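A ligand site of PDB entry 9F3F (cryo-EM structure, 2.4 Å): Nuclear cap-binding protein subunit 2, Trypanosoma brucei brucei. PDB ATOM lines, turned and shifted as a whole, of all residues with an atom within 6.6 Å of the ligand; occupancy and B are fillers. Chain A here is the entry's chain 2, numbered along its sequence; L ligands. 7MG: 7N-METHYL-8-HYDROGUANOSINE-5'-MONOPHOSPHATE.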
ATOM      1  N   MET A  12       4.285  17.319 -11.476  1.00  0.00           N
ATOM      2  CA  MET A  12       3.610  17.666 -10.207  1.00  0.00           C
ATOM      3  C   MET A  12       4.689  18.138  -9.224  1.00  0.00           C
ATOM      4  O   MET A  12       5.572  17.336  -8.883  1.00  0.00           O
ATOM      5  CB  MET A  12       2.903  16.434  -9.650  1.00  0.00           C
ATOM      6  CG  MET A  12       2.669  16.459  -8.161  1.00  0.00           C
ATOM      7  SD  MET A  12       1.837  14.947  -7.655  1.00  0.00           S
ATOM      8  CE  MET A  12       1.004  14.516  -9.177  1.00  0.00           C
ATOM      9  N   ALA A  13       4.645  19.410  -8.805  1.00  0.00           N
ATOM     10  CA  ALA A  13       5.722  19.994  -7.970  1.00  0.00           C
ATOM     11  C   ALA A  13       5.796  19.478  -6.537  1.00  0.00           C
ATOM     12  O   ALA A  13       6.935  19.214  -6.089  1.00  0.00           O
ATOM     13  CB  ALA A  13       5.549  21.493  -7.959  1.00  0.00           C
ATOM     14  N   TYR A  14       4.678  19.410  -5.813  1.00  0.00           N
ATOM     15  CA  TYR A  14       4.766  19.090  -4.365  1.00  0.00           C
ATOM     16  C   TYR A  14       5.087  17.613  -4.104  1.00  0.00           C
ATOM     17  O   TYR A  14       5.046  16.816  -5.046  1.00  0.00           O
ATOM     18  CB  TYR A  14       3.441  19.366  -3.644  1.00  0.00           C
ATOM     19  CG  TYR A  14       2.361  18.354  -3.916  1.00  0.00           C
ATOM     20  CD1 TYR A  14       1.875  18.129  -5.194  1.00  0.00           C
ATOM     21  CD2 TYR A  14       1.854  17.573  -2.892  1.00  0.00           C
ATOM     22  CE1 TYR A  14       0.897  17.178  -5.433  1.00  0.00           C
ATOM     23  CE2 TYR A  14       0.874  16.612  -3.118  1.00  0.00           C
ATOM     24  CZ  TYR A  14       0.400  16.422  -4.396  1.00  0.00           C
ATOM     25  OH  TYR A  14      -0.564  15.469  -4.635  1.00  0.00           O
ATOM     26  N   ASP A  16       4.313  14.319  -1.040  1.00  0.00           N
ATOM     27  CA  ASP A  16       3.299  14.033   0.006  1.00  0.00           C
ATOM     28  C   ASP A  16       3.816  12.908   0.899  1.00  0.00           C
ATOM     29  O   ASP A  16       4.716  12.163   0.462  1.00  0.00           O
ATOM     30  CB  ASP A  16       1.948  13.704  -0.638  1.00  0.00           C
ATOM     31  CG  ASP A  16       0.790  13.544   0.333  1.00  0.00           C
ATOM     32  OD1 ASP A  16       1.014  13.679   1.550  1.00  0.00           O
ATOM     33  OD2 ASP A  16      -0.333  13.282  -0.148  1.00  0.00           O
ATOM     34  N   HIS A  18       2.487  10.051   2.043  1.00  0.00           N
ATOM     35  CA  HIS A  18       2.346   8.639   1.586  1.00  0.00           C
ATOM     36  C   HIS A  18       3.496   8.403   0.608  1.00  0.00           C
ATOM     37  O   HIS A  18       4.093   7.308   0.645  1.00  0.00           O
ATOM     38  CB  HIS A  18       0.940   8.384   1.037  1.00  0.00           C
ATOM     39  CG  HIS A  18       0.617   9.071  -0.253  1.00  0.00           C
ATOM     40  ND1 HIS A  18       0.684  10.430  -0.436  1.00  0.00           N
ATOM     41  CD2 HIS A  18       0.222   8.557  -1.427  1.00  0.00           C
ATOM     42  CE1 HIS A  18       0.346  10.729  -1.684  1.00  0.00           C
ATOM     43  NE2 HIS A  18       0.057   9.599  -2.294  1.00  0.00           N
ATOM     44  N   LEU A  38       2.628   9.855 -14.097  1.00  0.00           N
ATOM     45  CA  LEU A  38       2.086  11.165 -14.533  1.00  0.00           C
ATOM     46  C   LEU A  38       2.126  11.281 -16.049  1.00  0.00           C
ATOM     47  O   LEU A  38       1.250  11.951 -16.602  1.00  0.00           O
ATOM     48  CB  LEU A  38       2.945  12.276 -13.942  1.00  0.00           C
ATOM     49  CG  LEU A  38       2.620  12.740 -12.528  1.00  0.00           C
ATOM     50  CD1 LEU A  38       3.603  13.804 -12.082  1.00  0.00           C
ATOM     51  CD2 LEU A  38       1.208  13.305 -12.485  1.00  0.00           C
ATOM     52  N   VAL A  44      -6.494  15.275 -12.899  1.00  0.00           N
ATOM     53  CA  VAL A  44      -6.088  16.668 -12.599  1.00  0.00           C
ATOM     54  C   VAL A  44      -6.633  17.038 -11.236  1.00  0.00           C
ATOM     55  O   VAL A  44      -7.708  16.533 -10.906  1.00  0.00           O
ATOM     56  CB  VAL A  44      -6.602  17.592 -13.715  1.00  0.00           C
ATOM     57  CG1 VAL A  44      -5.968  17.295 -15.060  1.00  0.00           C
ATOM     58  CG2 VAL A  44      -8.119  17.566 -13.829  1.00  0.00           C
ATOM     59  N   TYR A  45      -5.910  17.836 -10.466  1.00  0.00           N
ATOM     60  CA  TYR A  45      -6.389  18.358  -9.159  1.00  0.00           C
ATOM     61  C   TYR A  45      -6.969  19.716  -9.504  1.00  0.00           C
ATOM     62  O   TYR A  45      -6.319  20.432 -10.272  1.00  0.00           O
ATOM     63  CB  TYR A  45      -5.212  18.521  -8.212  1.00  0.00           C
ATOM     64  CG  TYR A  45      -5.535  18.944  -6.807  1.00  0.00           C
ATOM     65  CD1 TYR A  45      -6.290  18.156  -5.963  1.00  0.00           C
ATOM     66  CD2 TYR A  45      -5.128  20.179  -6.336  1.00  0.00           C
ATOM     67  CE1 TYR A  45      -6.581  18.547  -4.674  1.00  0.00           C
ATOM     68  CE2 TYR A  45      -5.414  20.597  -5.055  1.00  0.00           C
ATOM     69  CZ  TYR A  45      -6.145  19.774  -4.212  1.00  0.00           C
ATOM     70  OH  TYR A  45      -6.432  20.190  -2.941  1.00  0.00           O
ATOM     71  N   CYS A  83     -14.571  20.073   0.649  1.00  0.00           N
ATOM     72  CA  CYS A  83     -13.614  20.813   1.493  1.00  0.00           C
ATOM     73  C   CYS A  83     -12.766  21.804   0.702  1.00  0.00           C
ATOM     74  O   CYS A  83     -11.836  22.381   1.314  1.00  0.00           O
ATOM     75  CB  CYS A  83     -12.677  19.839   2.186  1.00  0.00           C
ATOM     76  SG  CYS A  83     -11.870  18.705   1.021  1.00  0.00           S
ATOM     77  N   PHE A  85     -11.480  21.365  -2.837  1.00  0.00           N
ATOM     78  CA  PHE A  85     -10.789  20.882  -4.077  1.00  0.00           C
ATOM     79  C   PHE A  85     -11.550  19.795  -4.761  1.00  0.00           C
ATOM     80  O   PHE A  85     -12.709  19.540  -4.409  1.00  0.00           O
ATOM     81  CB  PHE A  85      -9.456  20.218  -3.745  1.00  0.00           C
ATOM     82  CG  PHE A  85      -9.440  18.931  -2.928  1.00  0.00           C
ATOM     83  CD1 PHE A  85      -9.406  18.966  -1.542  1.00  0.00           C
ATOM     84  CD2 PHE A  85      -9.403  17.687  -3.553  1.00  0.00           C
ATOM     85  CE1 PHE A  85      -9.365  17.791  -0.811  1.00  0.00           C
ATOM     86  CE2 PHE A  85      -9.381  16.524  -2.815  1.00  0.00           C
ATOM     87  CZ  PHE A  85      -9.365  16.580  -1.444  1.00  0.00           C
ATOM     88  N   CYS A  86     -10.903  19.106  -5.689  1.00  0.00           N
ATOM     89  CA  CYS A  86     -11.577  18.059  -6.470  1.00  0.00           C
ATOM     90  C   CYS A  86     -10.560  17.273  -7.284  1.00  0.00           C
ATOM     91  O   CYS A  86      -9.376  17.652  -7.256  1.00  0.00           O
ATOM     92  CB  CYS A  86     -12.545  18.676  -7.474  1.00  0.00           C
ATOM     93  SG  CYS A  86     -13.637  17.500  -8.301  1.00  0.00           S
ATOM     94  N   PHE A  87     -10.976  16.199  -7.948  1.00  0.00           N
ATOM     95  CA  PHE A  87     -10.119  15.389  -8.824  1.00  0.00           C
ATOM     96  C   PHE A  87     -10.985  14.975 -10.006  1.00  0.00           C
ATOM     97  O   PHE A  87     -11.996  14.305  -9.796  1.00  0.00           O
ATOM     98  CB  PHE A  87      -9.552  14.134  -8.165  1.00  0.00           C
ATOM     99  CG  PHE A  87      -8.391  14.285  -7.214  1.00  0.00           C
ATOM    100  CD1 PHE A  87      -7.126  14.564  -7.680  1.00  0.00           C
ATOM    101  CD2 PHE A  87      -8.572  14.067  -5.863  1.00  0.00           C
ATOM    102  CE1 PHE A  87      -6.055  14.675  -6.809  1.00  0.00           C
ATOM    103  CE2 PHE A  87      -7.501  14.181  -4.983  1.00  0.00           C
ATOM    104  CZ  PHE A  87      -6.248  14.473  -5.462  1.00  0.00           C
ATOM    105  N   THR A 114      -7.126  26.243  -9.829  1.00  0.00           N
ATOM    106  CA  THR A 114      -5.691  25.973  -9.949  1.00  0.00           C
ATOM    107  C   THR A 114      -5.420  24.614 -10.566  1.00  0.00           C
ATOM    108  O   THR A 114      -4.639  23.827 -10.029  1.00  0.00           O
ATOM    109  CB  THR A 114      -5.006  26.053  -8.581  1.00  0.00           C
ATOM    110  OG1 THR A 114      -5.106  24.785  -7.933  1.00  0.00           O
ATOM    111  CG2 THR A 114      -5.641  27.111  -7.710  1.00  0.00           C
ATOM    112  N   SER A 116      -4.151  21.461 -12.086  1.00  0.00           N
ATOM    113  CA  SER A 116      -2.769  20.936 -12.140  1.00  0.00           C
ATOM    114  C   SER A 116      -2.816  19.477 -12.605  1.00  0.00           C
ATOM    115  O   SER A 116      -3.906  19.014 -12.965  1.00  0.00           O
ATOM    116  CB  SER A 116      -2.189  21.035 -10.785  1.00  0.00           C
ATOM    117  OG  SER A 116      -3.084  20.523  -9.810  1.00  0.00           O
ATOM    118  N   TRP A 117      -1.691  18.767 -12.610  1.00  0.00           N
ATOM    119  CA  TRP A 117      -1.594  17.365 -13.085  1.00  0.00           C
ATOM    120  C   TRP A 117      -1.408  16.459 -11.874  1.00  0.00           C
ATOM    121  O   TRP A 117      -0.521  16.773 -11.069  1.00  0.00           O
ATOM    122  CB  TRP A 117      -0.456  17.191 -14.082  1.00  0.00           C
ATOM    123  CG  TRP A 117      -0.644  17.612 -15.495  1.00  0.00           C
ATOM    124  CD1 TRP A 117      -0.204  18.773 -16.077  1.00  0.00           C
ATOM    125  CD2 TRP A 117      -1.209  16.830 -16.555  1.00  0.00           C
ATOM    126  NE1 TRP A 117      -0.513  18.775 -17.405  1.00  0.00           N
ATOM    127  CE2 TRP A 117      -1.129  17.600 -17.733  1.00  0.00           C
ATOM    128  CE3 TRP A 117      -1.815  15.566 -16.627  1.00  0.00           C
ATOM    129  CZ2 TRP A 117      -1.620  17.154 -18.956  1.00  0.00           C
ATOM    130  CZ3 TRP A 117      -2.291  15.123 -17.831  1.00  0.00           C
ATOM    131  CH2 TRP A 117      -2.203  15.908 -18.982  1.00  0.00           C
ATOM    132  N   ASP A 118      -2.221  15.423 -11.716  1.00  0.00           N
ATOM    133  CA  ASP A 118      -2.031  14.441 -10.608  1.00  0.00           C
ATOM    134  C   ASP A 118      -1.780  13.050 -11.194  1.00  0.00           C
ATOM    135  O   ASP A 118      -1.950  12.893 -12.406  1.00  0.00           O
ATOM    136  CB  ASP A 118      -3.173  14.446  -9.602  1.00  0.00           C
ATOM    137  CG  ASP A 118      -2.940  13.513  -8.436  1.00  0.00           C
ATOM    138  OD1 ASP A 118      -1.827  13.527  -7.892  1.00  0.00           O
ATOM    139  OD2 ASP A 118      -3.884  12.778  -8.083  1.00  0.00           O
ATOM    140  N   VAL A 119      -1.342  12.102 -10.372  1.00  0.00           N
ATOM    141  CA  VAL A 119      -1.005  10.732 -10.841  1.00  0.00           C
ATOM    142  C   VAL A 119      -2.286   9.919 -11.000  1.00  0.00           C
ATOM    143  O   VAL A 119      -2.407   9.198 -12.004  1.00  0.00           O
ATOM    144  CB  VAL A 119      -0.074  10.053  -9.818  1.00  0.00           C
ATOM    145  CG1 VAL A 119       0.108   8.574 -10.106  1.00  0.00           C
ATOM    146  CG2 VAL A 119       1.271  10.758  -9.713  1.00  0.00           C
ATOM    147  N   THR A 124      -8.576   7.280  -0.515  1.00  0.00           N
ATOM    148  CA  THR A 124      -7.782   7.959   0.518  1.00  0.00           C
ATOM    149  C   THR A 124      -7.529   9.388   0.112  1.00  0.00           C
ATOM    150  O   THR A 124      -7.681  10.271   0.971  1.00  0.00           O
ATOM    151  CB  THR A 124      -6.492   7.176   0.677  1.00  0.00           C
ATOM    152  OG1 THR A 124      -5.878   7.243  -0.608  1.00  0.00           O
ATOM    153  CG2 THR A 124      -6.741   5.731   1.057  1.00  0.00           C
ATOM    154  N   ARG A 125      -7.154   9.627  -1.146  1.00  0.00           N
ATOM    155  CA  ARG A 125      -6.808  10.989  -1.628  1.00  0.00           C
ATOM    156  C   ARG A 125      -8.048  11.892  -1.636  1.00  0.00           C
ATOM    157  O   ARG A 125      -7.882  13.104  -1.413  1.00  0.00           O
ATOM    158  CB  ARG A 125      -6.240  10.870  -3.035  1.00  0.00           C
ATOM    159  CG  ARG A 125      -4.998  10.008  -3.164  1.00  0.00           C
ATOM    160  CD  ARG A 125      -3.760  10.799  -2.779  1.00  0.00           C
ATOM    161  NE  ARG A 125      -3.573  12.018  -3.570  1.00  0.00           N
ATOM    162  CZ  ARG A 125      -3.328  12.093  -4.870  1.00  0.00           C
ATOM    163  NH1 ARG A 125      -3.488  11.041  -5.651  1.00  0.00           N
ATOM    164  NH2 ARG A 125      -2.887  13.223  -5.380  1.00  0.00           N
ATOM    165  N   ARG A 126      -9.234  11.330  -1.850  1.00  0.00           N
ATOM    166  CA  ARG A 126     -10.481  12.125  -1.951  1.00  0.00           C
ATOM    167  C   ARG A 126     -10.748  12.915  -0.687  1.00  0.00           C
ATOM    168  O   ARG A 126     -11.610  13.805  -0.721  1.00  0.00           O
ATOM    169  CB  ARG A 126     -11.678  11.199  -2.141  1.00  0.00           C
ATOM    170  CG  ARG A 126     -12.468  10.859  -0.886  1.00  0.00           C
ATOM    171  CD  ARG A 126     -13.838  10.299  -1.190  1.00  0.00           C
ATOM    172  NE  ARG A 126     -14.681  11.279  -1.887  1.00  0.00           N
ATOM    173  CZ  ARG A 126     -15.250  11.084  -3.058  1.00  0.00           C
ATOM    174  NH1 ARG A 126     -15.153   9.908  -3.652  1.00  0.00           N
ATOM    175  NH2 ARG A 126     -15.917  12.063  -3.644  1.00  0.00           N
ATOM    176  N   TRP A 127     -10.049  12.617   0.396  1.00  0.00           N
ATOM    177  CA  TRP A 127     -10.369  13.290   1.665  1.00  0.00           C
ATOM    178  C   TRP A 127      -9.370  14.388   1.955  1.00  0.00           C
ATOM    179  O   TRP A 127      -8.376  14.485   1.215  1.00  0.00           O
ATOM    180  CB  TRP A 127     -10.413  12.270   2.822  1.00  0.00           C
ATOM    181  CG  TRP A 127     -11.402  11.156   2.631  1.00  0.00           C
ATOM    182  CD1 TRP A 127     -11.166   9.954   2.020  1.00  0.00           C
ATOM    183  CD2 TRP A 127     -12.780  11.125   3.047  1.00  0.00           C
ATOM    184  NE1 TRP A 127     -12.299   9.194   2.020  1.00  0.00           N
ATOM    185  CE2 TRP A 127     -13.304   9.884   2.643  1.00  0.00           C
ATOM    186  CE3 TRP A 127     -13.618  12.035   3.716  1.00  0.00           C
ATOM    187  CZ2 TRP A 127     -14.627   9.527   2.893  1.00  0.00           C
ATOM    188  CZ3 TRP A 127     -14.927  11.673   3.957  1.00  0.00           C
ATOM    189  CH2 TRP A 127     -15.421  10.441   3.549  1.00  0.00           C
ATOM    190  N   GLY A 128      -9.612  15.173   2.990  1.00  0.00           N
ATOM    191  CA  GLY A 128      -8.703  16.255   3.381  1.00  0.00           C
ATOM    192  C   GLY A 128      -9.276  17.038   4.540  1.00  0.00           C
ATOM    193  O   GLY A 128     -10.389  16.675   4.975  1.00  0.00           O
HETATM  194  P   7MG L   1      -5.542  18.254   1.551  1.00  0.00           P
HETATM  195  OP1 7MG L   1      -6.923  18.782   1.239  1.00  0.00           O
HETATM  196  OP2 7MG L   1      -4.502  19.361   1.670  1.00  0.00           O
HETATM  197  OP3 7MG L   1      -5.519  17.306   2.737  1.00  0.00           O
HETATM  198  O5' 7MG L   1      -5.102  17.374   0.278  1.00  0.00           O
HETATM  199  C5' 7MG L   1      -5.925  16.246  -0.101  1.00  0.00           C
HETATM  200  C4' 7MG L   1      -5.343  15.603  -1.332  1.00  0.00           C
HETATM  201  O4' 7MG L   1      -5.149  16.641  -2.331  1.00  0.00           O
HETATM  202  C3' 7MG L   1      -3.972  14.939  -1.158  1.00  0.00           C
HETATM  203  O3' 7MG L   1      -4.108  13.525  -1.165  1.00  0.00           O
HETATM  204  C2' 7MG L   1      -3.083  15.483  -2.277  1.00  0.00           C
HETATM  205  O2' 7MG L   1      -2.557  14.470  -3.106  1.00  0.00           O
HETATM  206  C1' 7MG L   1      -4.020  16.336  -3.122  1.00  0.00           C
HETATM  207  N9  7MG L   1      -3.392  17.586  -3.536  1.00  0.00           N
HETATM  208  C8  7MG L   1      -3.317  18.753  -2.662  1.00  0.00           C
HETATM  209  N7  7MG L   1      -2.595  19.714  -3.494  1.00  0.00           N
HETATM  210  C5  7MG L   1      -2.269  19.135  -4.717  1.00  0.00           C
HETATM  211  C6  7MG L   1      -1.587  19.682  -5.812  1.00  0.00           C
HETATM  212  O6  7MG L   1      -1.107  20.793  -5.942  1.00  0.00           O
HETATM  213  N1  7MG L   1      -1.497  18.742  -6.840  1.00  0.00           N
HETATM  214  C2  7MG L   1      -1.993  17.463  -6.807  1.00  0.00           C
HETATM  215  N2  7MG L   1      -1.794  16.720  -7.896  1.00  0.00           N
HETATM  216  N3  7MG L   1      -2.637  16.971  -5.760  1.00  0.00           N
HETATM  217  C4  7MG L   1      -2.746  17.830  -4.739  1.00  0.00           C
HETATM  218  CM7 7MG L   1      -2.284  21.062  -3.043  1.00  0.00           C
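A nitrogen (N2) of the ligand sits close to the side-chain carboxylate (OD1) of Asp 118 (3.2 Å).
NH2 of Arg 125 sits at hydrogen-bond distance from O2' of the ligand (2.6 Å).
N2 of the ligand sits at hydrogen-bond distance from O of Trp 117 (3.4 Å).
The side-chain hydroxyl (OH) of Tyr 14 is in hydrogen-bond range of an oxygen (O2') of the ligand (2.7 Å).
The side-chain carboxylate (OD2) of Asp 16 is in hydrogen-bond range of a ring nitrogen (ND1) of His 18 (3.0 Å).
The backbone carbonyl oxygen (O) of Tyr 45 lies within hydrogen-bond range of the backbone NH (N) of Ser 116 (3.0 Å).
The guanidinium group of Arg 125 is in salt-bridge range of the side-chain carboxylate of Asp 118, 2.7 Å away.
The guanidinium group (NH2) of Arg 125 sits at hydrogen-bond distance from the side-chain hydroxyl (OH) of Tyr 14 (3.3 Å).
CE of Met 12 touches N2 of the ligand, at 3.8 Å.
Asp 16 touches the ligand.
Tyr 45 touches the ligand (CE2 to N7, 3.3 Å).
CE1 of Phe 85 touches OP1 of the ligand (3.3 Å).
Phe 87 touches the ligand (CZ to C1', 3.7 Å).
OG of Ser 116 touches N1 of the ligand, at 3.8 Å.
Trp 127 touches the ligand.
Gly 128 touches the ligand (CA to OP3, 3.4 Å).
Hydrophobic or aromatic side chains that line the ligand: Met 12, Tyr 14, Tyr 45, Phe 85 and Phe 87.
Of the 22 residues printed, 12 come within 4 Å of the ligand.
The nearest printed residue that does not touch the ligand is His 18 (4.9 Å).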
